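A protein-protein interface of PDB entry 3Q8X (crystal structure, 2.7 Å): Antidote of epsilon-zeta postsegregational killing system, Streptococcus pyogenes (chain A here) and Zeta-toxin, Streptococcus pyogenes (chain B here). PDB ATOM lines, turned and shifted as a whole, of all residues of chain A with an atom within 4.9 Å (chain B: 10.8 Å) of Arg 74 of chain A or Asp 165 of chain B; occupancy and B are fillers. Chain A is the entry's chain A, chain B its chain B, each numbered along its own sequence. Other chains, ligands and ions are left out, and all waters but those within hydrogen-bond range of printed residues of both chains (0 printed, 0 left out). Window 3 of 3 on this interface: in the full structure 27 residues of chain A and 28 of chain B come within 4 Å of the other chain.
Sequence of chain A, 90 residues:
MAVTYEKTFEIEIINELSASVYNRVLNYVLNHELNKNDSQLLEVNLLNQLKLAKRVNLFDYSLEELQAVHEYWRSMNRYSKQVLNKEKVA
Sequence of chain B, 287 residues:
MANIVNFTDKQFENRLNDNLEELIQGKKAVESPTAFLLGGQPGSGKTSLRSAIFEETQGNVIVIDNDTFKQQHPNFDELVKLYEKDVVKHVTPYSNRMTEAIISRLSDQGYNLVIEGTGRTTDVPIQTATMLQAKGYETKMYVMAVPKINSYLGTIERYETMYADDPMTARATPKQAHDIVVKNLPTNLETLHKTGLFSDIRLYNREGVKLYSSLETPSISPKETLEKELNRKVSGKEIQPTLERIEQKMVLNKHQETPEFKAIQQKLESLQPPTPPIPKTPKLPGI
NE2 of His 70 of chain A sits close to NH2 of Arg 74 of chain A, at 3.2 Å.
NH1 of Arg 74 of chain A is in salt-bridge range of OE1 of Glu 71 of chain A (2.8 Å).
The backbone carbonyl oxygen (O) of Glu 157 of chain B is in hydrogen-bond range of the side-chain hydroxyl (OG1) of Thr 161 of chain B (2.9 Å).
The backbone NH of Met 168 of chain B is in hydrogen-bond range of the side-chain carboxylate of Asp 166 of chain B (3.2 Å).
The side-chain carboxylate (OD2) of Asp 166 of chain B is in hydrogen-bond range of the side-chain hydroxyl (OG1) of Thr 169 of chain B, 3.4 Å away.
A ring nitrogen (NE2) of His 70 of chain A is in hydrogen-bond range of the side-chain carboxylate of Asp 165 of chain B (2.5 Å).
The side-chain carboxylate of Asp 165 of chain B is in salt-bridge range of the guanidinium group of Arg 74 of chain A.
The side-chain amide nitrogen of Asn 77 of chain A sits at hydrogen-bond distance from the side-chain carboxylate of Asp 166 of chain B.
Along chain B the printed residues that touch a printed residue of chain A span positions 161 to 166.
Printed residues of chain A that touch a printed residue of chain B: Ile 13, Leu 17, His 70, Arg 74 and Asn 77.
Among the printed residues, 5 pairs touch across the chains.
Among the printed residues, Asp or Glu carboxylates within 4 Å of a Lys or Arg side-chain nitrogen of the other chain: Arg 74 of chain A with Asp 165 of chain B.
Thr 161 of chain B touches Ile 13 of chain A (CG2 to CG1, 3.9 Å).
Asp 165 of chain B touches Leu 17 of chain A (OD2 to CD2, 3.9 Å).
Arg 74 of chain A touches just one residue of chain B: Asp 165.
Of the printed residues of chain A, Asp 165 of chain B touches Leu 17, His 70 and Arg 74.
No residue of chain B comes within 4 Å of Glu 71 of chain A.
No residue of chain B comes within 4 Å of Ser 75 of chain A.
No residue of chain B comes within 4 Å of Arg 78 of chain A.
Of the printed residues of chain A, Asp 166 of chain B touches Asn 77.
Of the printed residues of chain B, Ile 13 of chain A touches Thr 161.
Printed residues of chain A within 4 Å of Thr 161 of chain B: Ile 13 (3.9 Å).
Of the printed residues of chain B, Leu 17 of chain A touches Asp 165 (3.9 Å).
The nearest residue of chain B that does not touch Arg 74 of chain A is Ala 164 of chain B (5.7 Å).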
ATOM      1  N   ILE A  13      19.117  -0.436  -6.321  1.00  0.00           N
ATOM      2  CA  ILE A  13      18.518  -0.489  -7.647  1.00  0.00           C
ATOM      3  C   ILE A  13      18.549   0.897  -8.300  1.00  0.00           C
ATOM      4  O   ILE A  13      18.921   1.021  -9.475  1.00  0.00           O
ATOM      5  CB  ILE A  13      17.091  -1.099  -7.597  1.00  0.00           C
ATOM      6  CG1 ILE A  13      17.130  -2.603  -7.896  1.00  0.00           C
ATOM      7  CG2 ILE A  13      16.194  -0.480  -8.636  1.00  0.00           C
ATOM      8  CD1 ILE A  13      17.931  -3.439  -6.941  1.00  0.00           C
ATOM      9  N   LEU A  17      20.379   1.837 -11.929  1.00  0.00           N
ATOM     10  CA  LEU A  17      19.582   2.459 -12.984  1.00  0.00           C
ATOM     11  C   LEU A  17      20.023   3.876 -13.309  1.00  0.00           C
ATOM     12  O   LEU A  17      20.227   4.197 -14.473  1.00  0.00           O
ATOM     13  CB  LEU A  17      18.086   2.434 -12.666  1.00  0.00           C
ATOM     14  CG  LEU A  17      17.200   2.932 -13.810  1.00  0.00           C
ATOM     15  CD1 LEU A  17      17.316   2.038 -15.035  1.00  0.00           C
ATOM     16  CD2 LEU A  17      15.776   3.028 -13.379  1.00  0.00           C
ATOM     17  N   HIS A  70      13.105   6.406  -7.705  1.00  0.00           N
ATOM     18  CA  HIS A  70      13.128   5.266  -8.612  1.00  0.00           C
ATOM     19  C   HIS A  70      12.319   5.527  -9.906  1.00  0.00           C
ATOM     20  O   HIS A  70      12.839   5.357 -11.006  1.00  0.00           O
ATOM     21  CB  HIS A  70      12.582   4.037  -7.885  1.00  0.00           C
ATOM     22  CG  HIS A  70      12.839   2.748  -8.595  1.00  0.00           C
ATOM     23  ND1 HIS A  70      12.790   1.528  -7.954  1.00  0.00           N
ATOM     24  CD2 HIS A  70      13.166   2.485  -9.882  1.00  0.00           C
ATOM     25  CE1 HIS A  70      13.057   0.568  -8.821  1.00  0.00           C
ATOM     26  NE2 HIS A  70      13.290   1.122  -9.999  1.00  0.00           N
ATOM     27  N   GLU A  71      11.059   5.949  -9.770  1.00  0.00           N
ATOM     28  CA  GLU A  71      10.216   6.222 -10.933  1.00  0.00           C
ATOM     29  C   GLU A  71      10.686   7.433 -11.733  1.00  0.00           C
ATOM     30  O   GLU A  71      10.404   7.532 -12.931  1.00  0.00           O
ATOM     31  CB  GLU A  71       8.745   6.370 -10.540  1.00  0.00           C
ATOM     32  CG  GLU A  71       7.800   6.800 -11.687  1.00  0.00           C
ATOM     33  CD  GLU A  71       7.797   5.857 -12.908  1.00  0.00           C
ATOM     34  OE1 GLU A  71       8.205   4.674 -12.774  1.00  0.00           O
ATOM     35  OE2 GLU A  71       7.370   6.311 -14.000  1.00  0.00           O
ATOM     36  N   TYR A  72      11.413   8.341 -11.088  1.00  0.00           N
ATOM     37  CA  TYR A  72      12.120   9.379 -11.829  1.00  0.00           C
ATOM     38  C   TYR A  72      13.101   8.764 -12.829  1.00  0.00           C
ATOM     39  O   TYR A  72      13.074   9.103 -14.003  1.00  0.00           O
ATOM     40  CB  TYR A  72      12.863  10.336 -10.895  1.00  0.00           C
ATOM     41  CG  TYR A  72      13.727  11.325 -11.634  1.00  0.00           C
ATOM     42  CD1 TYR A  72      13.175  12.473 -12.192  1.00  0.00           C
ATOM     43  CD2 TYR A  72      15.093  11.098 -11.798  1.00  0.00           C
ATOM     44  CE1 TYR A  72      13.965  13.383 -12.892  1.00  0.00           C
ATOM     45  CE2 TYR A  72      15.899  11.999 -12.479  1.00  0.00           C
ATOM     46  CZ  TYR A  72      15.333  13.141 -13.030  1.00  0.00           C
ATOM     47  OH  TYR A  72      16.123  14.041 -13.720  1.00  0.00           O
ATOM     48  N   TRP A  73      13.962   7.866 -12.362  1.00  0.00           N
ATOM     49  CA  TRP A  73      14.954   7.255 -13.243  1.00  0.00           C
ATOM     50  C   TRP A  73      14.372   6.292 -14.279  1.00  0.00           C
ATOM     51  O   TRP A  73      14.987   6.085 -15.334  1.00  0.00           O
ATOM     52  CB  TRP A  73      16.090   6.610 -12.452  1.00  0.00           C
ATOM     53  CG  TRP A  73      16.915   7.643 -11.720  1.00  0.00           C
ATOM     54  CD1 TRP A  73      16.818   7.987 -10.404  1.00  0.00           C
ATOM     55  CD2 TRP A  73      17.936   8.490 -12.280  1.00  0.00           C
ATOM     56  NE1 TRP A  73      17.728   8.976 -10.105  1.00  0.00           N
ATOM     57  CE2 TRP A  73      18.417   9.307 -11.237  1.00  0.00           C
ATOM     58  CE3 TRP A  73      18.489   8.631 -13.564  1.00  0.00           C
ATOM     59  CZ2 TRP A  73      19.427  10.245 -11.431  1.00  0.00           C
ATOM     60  CZ3 TRP A  73      19.487   9.564 -13.761  1.00  0.00           C
ATOM     61  CH2 TRP A  73      19.948  10.361 -12.701  1.00  0.00           C
ATOM     62  N   ARG A  74      13.192   5.725 -14.018  1.00  0.00           N
ATOM     63  CA  ARG A  74      12.530   4.929 -15.057  1.00  0.00           C
ATOM     64  C   ARG A  74      12.134   5.868 -16.188  1.00  0.00           C
ATOM     65  O   ARG A  74      12.293   5.563 -17.381  1.00  0.00           O
ATOM     66  CB  ARG A  74      11.294   4.209 -14.520  1.00  0.00           C
ATOM     67  CG  ARG A  74      11.584   3.117 -13.521  1.00  0.00           C
ATOM     68  CD  ARG A  74      10.400   2.179 -13.336  1.00  0.00           C
ATOM     69  NE  ARG A  74      10.537   1.481 -12.060  1.00  0.00           N
ATOM     70  CZ  ARG A  74       9.883   1.796 -10.944  1.00  0.00           C
ATOM     71  NH1 ARG A  74       8.995   2.787 -10.932  1.00  0.00           N
ATOM     72  NH2 ARG A  74      10.111   1.109  -9.836  1.00  0.00           N
ATOM     73  N   SER A  75      11.636   7.030 -15.777  1.00  0.00           N
ATOM     74  CA  SER A  75      11.165   8.065 -16.677  1.00  0.00           C
ATOM     75  C   SER A  75      12.293   8.624 -17.544  1.00  0.00           C
ATOM     76  O   SER A  75      12.134   8.757 -18.762  1.00  0.00           O
ATOM     77  CB  SER A  75      10.479   9.179 -15.878  1.00  0.00           C
ATOM     78  OG  SER A  75       9.919  10.148 -16.737  1.00  0.00           O
ATOM     79  N   MET A  76      13.431   8.939 -16.932  1.00  0.00           N
ATOM     80  CA  MET A  76      14.558   9.451 -17.713  1.00  0.00           C
ATOM     81  C   MET A  76      15.138   8.362 -18.596  1.00  0.00           C
ATOM     82  O   MET A  76      15.502   8.629 -19.729  1.00  0.00           O
ATOM     83  CB  MET A  76      15.642  10.098 -16.848  1.00  0.00           C
ATOM     84  CG  MET A  76      15.223  11.391 -16.187  1.00  0.00           C
ATOM     85  SD  MET A  76      14.439  12.542 -17.329  1.00  0.00           S
ATOM     86  CE  MET A  76      14.797  14.099 -16.515  1.00  0.00           C
ATOM     87  N   ASN A  77      15.200   7.131 -18.095  1.00  0.00           N
ATOM     88  CA  ASN A  77      15.586   6.006 -18.940  1.00  0.00           C
ATOM     89  C   ASN A  77      14.737   5.926 -20.213  1.00  0.00           C
ATOM     90  O   ASN A  77      15.283   5.858 -21.327  1.00  0.00           O
ATOM     91  CB  ASN A  77      15.530   4.689 -18.167  1.00  0.00           C
ATOM     92  CG  ASN A  77      16.098   3.527 -18.958  1.00  0.00           C
ATOM     93  OD1 ASN A  77      17.143   3.646 -19.587  1.00  0.00           O
ATOM     94  ND2 ASN A  77      15.406   2.395 -18.933  1.00  0.00           N
ATOM     95  N   ARG A  78      13.414   5.956 -20.050  1.00  0.00           N
ATOM     96  CA  ARG A  78      12.493   5.971 -21.199  1.00  0.00           C
ATOM     97  C   ARG A  78      12.749   7.154 -22.126  1.00  0.00           C
ATOM     98  O   ARG A  78      12.871   6.991 -23.340  1.00  0.00           O
ATOM     99  CB  ARG A  78      11.029   5.996 -20.746  1.00  0.00           C
ATOM    100  CG  ARG A  78      10.424   4.631 -20.529  1.00  0.00           C
ATOM    101  CD  ARG A  78       8.923   4.738 -20.330  1.00  0.00           C
ATOM    102  NE  ARG A  78       8.553   5.592 -19.198  1.00  0.00           N
ATOM    103  CZ  ARG A  78       8.437   5.174 -17.938  1.00  0.00           C
ATOM    104  NH1 ARG A  78       8.669   3.901 -17.628  1.00  0.00           N
ATOM    105  NH2 ARG A  78       8.090   6.031 -16.981  1.00  0.00           N
ATOM    106  N   GLU B 157      16.412 -11.317  -6.844  1.00  0.00           N
ATOM    107  CA  GLU B 157      15.489 -10.193  -6.766  1.00  0.00           C
ATOM    108  C   GLU B 157      16.040  -8.972  -7.498  1.00  0.00           C
ATOM    109  O   GLU B 157      15.314  -8.291  -8.232  1.00  0.00           O
ATOM    110  CB  GLU B 157      15.171  -9.846  -5.306  1.00  0.00           C
ATOM    111  CG  GLU B 157      14.128  -8.737  -5.144  1.00  0.00           C
ATOM    112  CD  GLU B 157      13.751  -8.469  -3.701  1.00  0.00           C
ATOM    113  OE1 GLU B 157      14.356  -9.086  -2.793  1.00  0.00           O
ATOM    114  OE2 GLU B 157      12.835  -7.647  -3.473  1.00  0.00           O
ATOM    115  N   ARG B 158      17.324  -8.701  -7.280  1.00  0.00           N
ATOM    116  CA  ARG B 158      17.998  -7.597  -7.931  1.00  0.00           C
ATOM    117  C   ARG B 158      17.798  -7.738  -9.421  1.00  0.00           C
ATOM    118  O   ARG B 158      17.262  -6.833 -10.076  1.00  0.00           O
ATOM    119  CB  ARG B 158      19.478  -7.637  -7.609  1.00  0.00           C
ATOM    120  CG  ARG B 158      20.298  -6.608  -8.336  1.00  0.00           C
ATOM    121  CD  ARG B 158      21.732  -6.780  -7.926  1.00  0.00           C
ATOM    122  NE  ARG B 158      22.677  -6.212  -8.881  1.00  0.00           N
ATOM    123  CZ  ARG B 158      22.965  -6.728 -10.079  1.00  0.00           C
ATOM    124  NH1 ARG B 158      22.353  -7.839 -10.522  1.00  0.00           N
ATOM    125  NH2 ARG B 158      23.867  -6.110 -10.847  1.00  0.00           N
ATOM    126  N   TYR B 159      18.197  -8.894  -9.947  1.00  0.00           N
ATOM    127  CA  TYR B 159      18.068  -9.159 -11.364  1.00  0.00           C
ATOM    128  C   TYR B 159      16.635  -8.938 -11.889  1.00  0.00           C
ATOM    129  O   TYR B 159      16.442  -8.274 -12.908  1.00  0.00           O
ATOM    130  CB  TYR B 159      18.578 -10.560 -11.692  1.00  0.00           C
ATOM    131  CG  TYR B 159      18.210 -11.002 -13.077  1.00  0.00           C
ATOM    132  CD1 TYR B 159      18.712 -10.335 -14.193  1.00  0.00           C
ATOM    133  CD2 TYR B 159      17.337 -12.064 -13.279  1.00  0.00           C
ATOM    134  CE1 TYR B 159      18.368 -10.732 -15.471  1.00  0.00           C
ATOM    135  CE2 TYR B 159      16.991 -12.466 -14.557  1.00  0.00           C
ATOM    136  CZ  TYR B 159      17.512 -11.793 -15.645  1.00  0.00           C
ATOM    137  OH  TYR B 159      17.173 -12.174 -16.920  1.00  0.00           O
ATOM    138  N   GLU B 160      15.637  -9.481 -11.197  1.00  0.00           N
ATOM    139  CA  GLU B 160      14.261  -9.398 -11.685  1.00  0.00           C
ATOM    140  C   GLU B 160      13.650  -8.001 -11.543  1.00  0.00           C
ATOM    141  O   GLU B 160      12.747  -7.640 -12.302  1.00  0.00           O
ATOM    142  CB  GLU B 160      13.372 -10.447 -11.023  1.00  0.00           C
ATOM    143  CG  GLU B 160      13.808 -11.886 -11.287  1.00  0.00           C
ATOM    144  CD  GLU B 160      13.539 -12.367 -12.710  1.00  0.00           C
ATOM    145  OE1 GLU B 160      12.646 -11.817 -13.389  1.00  0.00           O
ATOM    146  OE2 GLU B 160      14.224 -13.317 -13.144  1.00  0.00           O
ATOM    147  N   THR B 161      14.148  -7.215 -10.590  1.00  0.00           N
ATOM    148  CA  THR B 161      13.695  -5.833 -10.421  1.00  0.00           C
ATOM    149  C   THR B 161      14.313  -4.940 -11.477  1.00  0.00           C
ATOM    150  O   THR B 161      13.676  -3.990 -11.948  1.00  0.00           O
ATOM    151  CB  THR B 161      14.015  -5.297  -9.013  1.00  0.00           C
ATOM    152  OG1 THR B 161      13.392  -6.148  -8.041  1.00  0.00           O
ATOM    153  CG2 THR B 161      13.505  -3.864  -8.829  1.00  0.00           C
ATOM    154  N   MET B 162      15.553  -5.260 -11.842  1.00  0.00           N
ATOM    155  CA  MET B 162      16.269  -4.547 -12.892  1.00  0.00           C
ATOM    156  C   MET B 162      15.661  -4.834 -14.245  1.00  0.00           C
ATOM    157  O   MET B 162      15.447  -3.925 -15.049  1.00  0.00           O
ATOM    158  CB  MET B 162      17.747  -4.923 -12.894  1.00  0.00           C
ATOM    159  CG  MET B 162      18.614  -4.053 -11.963  1.00  0.00           C
ATOM    160  SD  MET B 162      20.328  -4.682 -11.932  1.00  0.00           S
ATOM    161  CE  MET B 162      21.010  -3.881 -13.410  1.00  0.00           C
ATOM    162  N   TYR B 163      15.364  -6.108 -14.481  1.00  0.00           N
ATOM    163  CA  TYR B 163      14.746  -6.546 -15.728  1.00  0.00           C
ATOM    164  C   TYR B 163      13.409  -5.847 -15.947  1.00  0.00           C
ATOM    165  O   TYR B 163      13.080  -5.473 -17.072  1.00  0.00           O
ATOM    166  CB  TYR B 163      14.566  -8.064 -15.724  1.00  0.00           C
ATOM    167  CG  TYR B 163      14.103  -8.614 -17.043  1.00  0.00           C
ATOM    168  CD1 TYR B 163      12.754  -8.581 -17.402  1.00  0.00           C
ATOM    169  CD2 TYR B 163      15.011  -9.168 -17.939  1.00  0.00           C
ATOM    170  CE1 TYR B 163      12.321  -9.077 -18.626  1.00  0.00           C
ATOM    171  CE2 TYR B 163      14.587  -9.675 -19.164  1.00  0.00           C
ATOM    172  CZ  TYR B 163      13.245  -9.623 -19.498  1.00  0.00           C
ATOM    173  OH  TYR B 163      12.833 -10.124 -20.703  1.00  0.00           O
ATOM    174  N   ALA B 164      12.651  -5.676 -14.865  1.00  0.00           N
ATOM    175  CA  ALA B 164      11.351  -5.012 -14.907  1.00  0.00           C
ATOM    176  C   ALA B 164      11.470  -3.528 -15.258  1.00  0.00           C
ATOM    177  O   ALA B 164      10.567  -2.963 -15.878  1.00  0.00           O
ATOM    178  CB  ALA B 164      10.612  -5.195 -13.593  1.00  0.00           C
ATOM    179  N   ASP B 165      12.580  -2.907 -14.858  1.00  0.00           N
ATOM    180  CA  ASP B 165      12.874  -1.535 -15.244  1.00  0.00           C
ATOM    181  C   ASP B 165      13.414  -1.506 -16.664  1.00  0.00           C
ATOM    182  O   ASP B 165      12.915  -0.754 -17.506  1.00  0.00           O
ATOM    183  CB  ASP B 165      13.872  -0.893 -14.280  1.00  0.00           C
ATOM    184  CG  ASP B 165      13.268  -0.605 -12.918  1.00  0.00           C
ATOM    185  OD1 ASP B 165      12.041  -0.761 -12.762  1.00  0.00           O
ATOM    186  OD2 ASP B 165      14.021  -0.226 -11.998  1.00  0.00           O
ATOM    187  N   ASP B 166      14.416  -2.349 -16.926  1.00  0.00           N
ATOM    188  CA  ASP B 166      15.078  -2.398 -18.225  1.00  0.00           C
ATOM    189  C   ASP B 166      15.680  -3.775 -18.523  1.00  0.00           C
ATOM    190  O   ASP B 166      16.674  -4.170 -17.903  1.00  0.00           O
ATOM    191  CB  ASP B 166      16.156  -1.308 -18.313  1.00  0.00           C
ATOM    192  CG  ASP B 166      16.532  -0.977 -19.742  1.00  0.00           C
ATOM    193  OD1 ASP B 166      16.325  -1.829 -20.636  1.00  0.00           O
ATOM    194  OD2 ASP B 166      17.036   0.142 -19.976  1.00  0.00           O
ATOM    195  N   PRO B 167      15.061  -4.518 -19.461  1.00  0.00           N
ATOM    196  CA  PRO B 167      15.551  -5.822 -19.927  1.00  0.00           C
ATOM    197  C   PRO B 167      16.986  -5.841 -20.495  1.00  0.00           C
ATOM    198  O   PRO B 167      17.706  -6.815 -20.266  1.00  0.00           O
ATOM    199  CB  PRO B 167      14.528  -6.213 -20.992  1.00  0.00           C
ATOM    200  CG  PRO B 167      13.287  -5.496 -20.573  1.00  0.00           C
ATOM    201  CD  PRO B 167      13.780  -4.172 -20.100  1.00  0.00           C
ATOM    202  N   MET B 168      17.404  -4.794 -21.210  1.00  0.00           N
ATOM    203  CA  MET B 168      18.759  -4.746 -21.786  1.00  0.00           C
ATOM    204  C   MET B 168      19.837  -4.636 -20.701  1.00  0.00           C
ATOM    205  O   MET B 168      20.835  -5.353 -20.720  1.00  0.00           O
ATOM    206  CB  MET B 168      18.907  -3.574 -22.758  1.00  0.00           C
ATOM    207  CG  MET B 168      17.786  -3.425 -23.782  1.00  0.00           C
ATOM    208  SD  MET B 168      18.084  -2.083 -24.982  1.00  0.00           S
ATOM    209  CE  MET B 168      18.688  -0.724 -23.952  1.00  0.00           C
ATOM    210  N   THR B 169      19.600  -3.724 -19.761  1.00  0.00           N
ATOM    211  CA  THR B 169      20.519  -3.380 -18.679  1.00  0.00           C
ATOM    212  C   THR B 169      20.688  -4.504 -17.639  1.00  0.00           C
ATOM    213  O   THR B 169      21.739  -4.618 -17.006  1.00  0.00           O
ATOM    214  CB  THR B 169      20.027  -2.072 -17.999  1.00  0.00           C
ATOM    215  OG1 THR B 169      20.084  -0.999 -18.949  1.00  0.00           O
ATOM    216  CG2 THR B 169      20.846  -1.705 -16.744  1.00  0.00           C
ATOM    217  N   ALA B 170      19.660  -5.331 -17.471  1.00  0.00           N
ATOM    218  CA  ALA B 170      19.679  -6.375 -16.450  1.00  0.00           C
ATOM    219  C   ALA B 170      20.564  -7.548 -16.836  1.00  0.00           C
ATOM    220  O   ALA B 170      20.407  -8.121 -17.918  1.00  0.00           O
ATOM    221  CB  ALA B 170      18.267  -6.860 -16.155  1.00  0.00           C
ATOM    222  N   ARG B 171      21.493  -7.896 -15.947  1.00  0.00           N
ATOM    223  CA  ARG B 171      22.306  -9.110 -16.097  1.00  0.00           C
ATOM    224  C   ARG B 171      22.288  -9.933 -14.815  1.00  0.00           C
ATOM    225  O   ARG B 171      22.567  -9.426 -13.731  1.00  0.00           O
ATOM    226  CB  ARG B 171      23.752  -8.783 -16.511  1.00  0.00           C
ATOM    227  CG  ARG B 171      23.867  -8.090 -17.865  1.00  0.00           C
ATOM    228  CD  ARG B 171      25.225  -7.454 -18.054  1.00  0.00           C
ATOM    229  NE  ARG B 171      25.118  -6.087 -18.572  1.00  0.00           N
ATOM    230  CZ  ARG B 171      25.525  -4.990 -17.923  1.00  0.00           C
ATOM    231  NH1 ARG B 171      26.088  -5.066 -16.717  1.00  0.00           N
ATOM    232  NH2 ARG B 171      25.377  -3.801 -18.492  1.00  0.00           N
ATOM    233  N   GLN B 248       6.364 -11.878  -7.661  1.00  0.00           N
ATOM    234  CA  GLN B 248       5.646 -10.732  -8.203  1.00  0.00           C
ATOM    235  C   GLN B 248       6.325 -10.153  -9.446  1.00  0.00           C
ATOM    236  O   GLN B 248       5.676  -9.921 -10.470  1.00  0.00           O
ATOM    237  CB  GLN B 248       5.509  -9.645  -7.137  1.00  0.00           C
ATOM    238  CG  GLN B 248       4.363  -8.714  -7.412  1.00  0.00           C
ATOM    239  CD  GLN B 248       4.758  -7.267  -7.385  1.00  0.00           C
ATOM    240  OE1 GLN B 248       5.815  -6.884  -7.898  1.00  0.00           O
ATOM    241  NE2 GLN B 248       3.894  -6.434  -6.806  1.00  0.00           N
ATOM    242  N   LYS B 249       7.628  -9.923  -9.336  1.00  0.00           N
ATOM    243  CA  LYS B 249       8.426  -9.413 -10.439  1.00  0.00           C
ATOM    244  C   LYS B 249       8.587 -10.466 -11.542  1.00  0.00           C
ATOM    245  O   LYS B 249       8.553 -10.133 -12.724  1.00  0.00           O
ATOM    246  CB  LYS B 249       9.801  -8.948  -9.937  1.00  0.00           C
ATOM    247  CG  LYS B 249       9.762  -7.742  -9.011  1.00  0.00           C
ATOM    248  CD  LYS B 249       9.780  -6.427  -9.802  1.00  0.00           C
ATOM    249  CE  LYS B 249       9.222  -5.256  -8.974  1.00  0.00           C
ATOM    250  NZ  LYS B 249       7.715  -5.292  -8.956  1.00  0.00           N
ATOM    251  N   MET B 250       8.754 -11.730 -11.159  1.00  0.00           N
ATOM    252  CA  MET B 250       8.944 -12.783 -12.144  1.00  0.00           C
ATOM    253  C   MET B 250       7.696 -12.984 -12.976  1.00  0.00           C
ATOM    254  O   MET B 250       7.789 -13.176 -14.189  1.00  0.00           O
ATOM    255  CB  MET B 250       9.398 -14.090 -11.489  1.00  0.00           C
ATOM    256  CG  MET B 250      10.850 -14.022 -10.974  1.00  0.00           C
ATOM    257  SD  MET B 250      11.618 -15.593 -10.504  1.00  0.00           S
ATOM    258  CE  MET B 250      11.816 -16.396 -12.100  1.00  0.00           C
ATOM    259  N   LEU B 252       5.378 -10.618 -13.550  1.00  0.00           N
ATOM    260  CA  LEU B 252       5.378  -9.423 -14.395  1.00  0.00           C
ATOM    261  C   LEU B 252       6.357  -9.547 -15.578  1.00  0.00           C
ATOM    262  O   LEU B 252       6.023  -9.194 -16.709  1.00  0.00           O
ATOM    263  CB  LEU B 252       5.655  -8.164 -13.549  1.00  0.00           C
ATOM    264  CG  LEU B 252       6.047  -6.840 -14.227  1.00  0.00           C
ATOM    265  CD1 LEU B 252       4.925  -6.249 -15.101  1.00  0.00           C
ATOM    266  CD2 LEU B 252       6.541  -5.821 -13.203  1.00  0.00           C
ATOM    267  N   ASN B 253       7.549 -10.070 -15.315  1.00  0.00           N
ATOM    268  CA  ASN B 253       8.575 -10.237 -16.345  1.00  0.00           C
ATOM    269  C   ASN B 253       8.341 -11.449 -17.249  1.00  0.00           C
ATOM    270  O   ASN B 253       9.121 -11.696 -18.172  1.00  0.00           O
ATOM    271  CB  ASN B 253       9.961 -10.311 -15.704  1.00  0.00           C
ATOM    272  CG  ASN B 253      10.329  -9.036 -14.975  1.00  0.00           C
ATOM    273  OD1 ASN B 253       9.840  -7.963 -15.311  1.00  0.00           O
ATOM    274  ND2 ASN B 253      11.202  -9.144 -13.984  1.00  0.00           N
ATOM    275  N   HIS B 255       8.634 -14.611 -16.442  1.00  0.00           N
ATOM    276  CA  HIS B 255       9.699 -15.588 -16.232  1.00  0.00           C
ATOM    277  C   HIS B 255       9.216 -16.787 -15.426  1.00  0.00           C
ATOM    278  O   HIS B 255       9.966 -17.350 -14.639  1.00  0.00           O
ATOM    279  CB  HIS B 255      10.921 -14.954 -15.556  1.00  0.00           C
ATOM    280  CG  HIS B 255      11.628 -13.945 -16.405  1.00  0.00           C
ATOM    281  ND1 HIS B 255      12.615 -13.118 -15.909  1.00  0.00           N
ATOM    282  CD2 HIS B 255      11.481 -13.614 -17.709  1.00  0.00           C
ATOM    283  CE1 HIS B 255      13.049 -12.328 -16.874  1.00  0.00           C
ATOM    284  NE2 HIS B 255      12.375 -12.605 -17.974  1.00  0.00           N
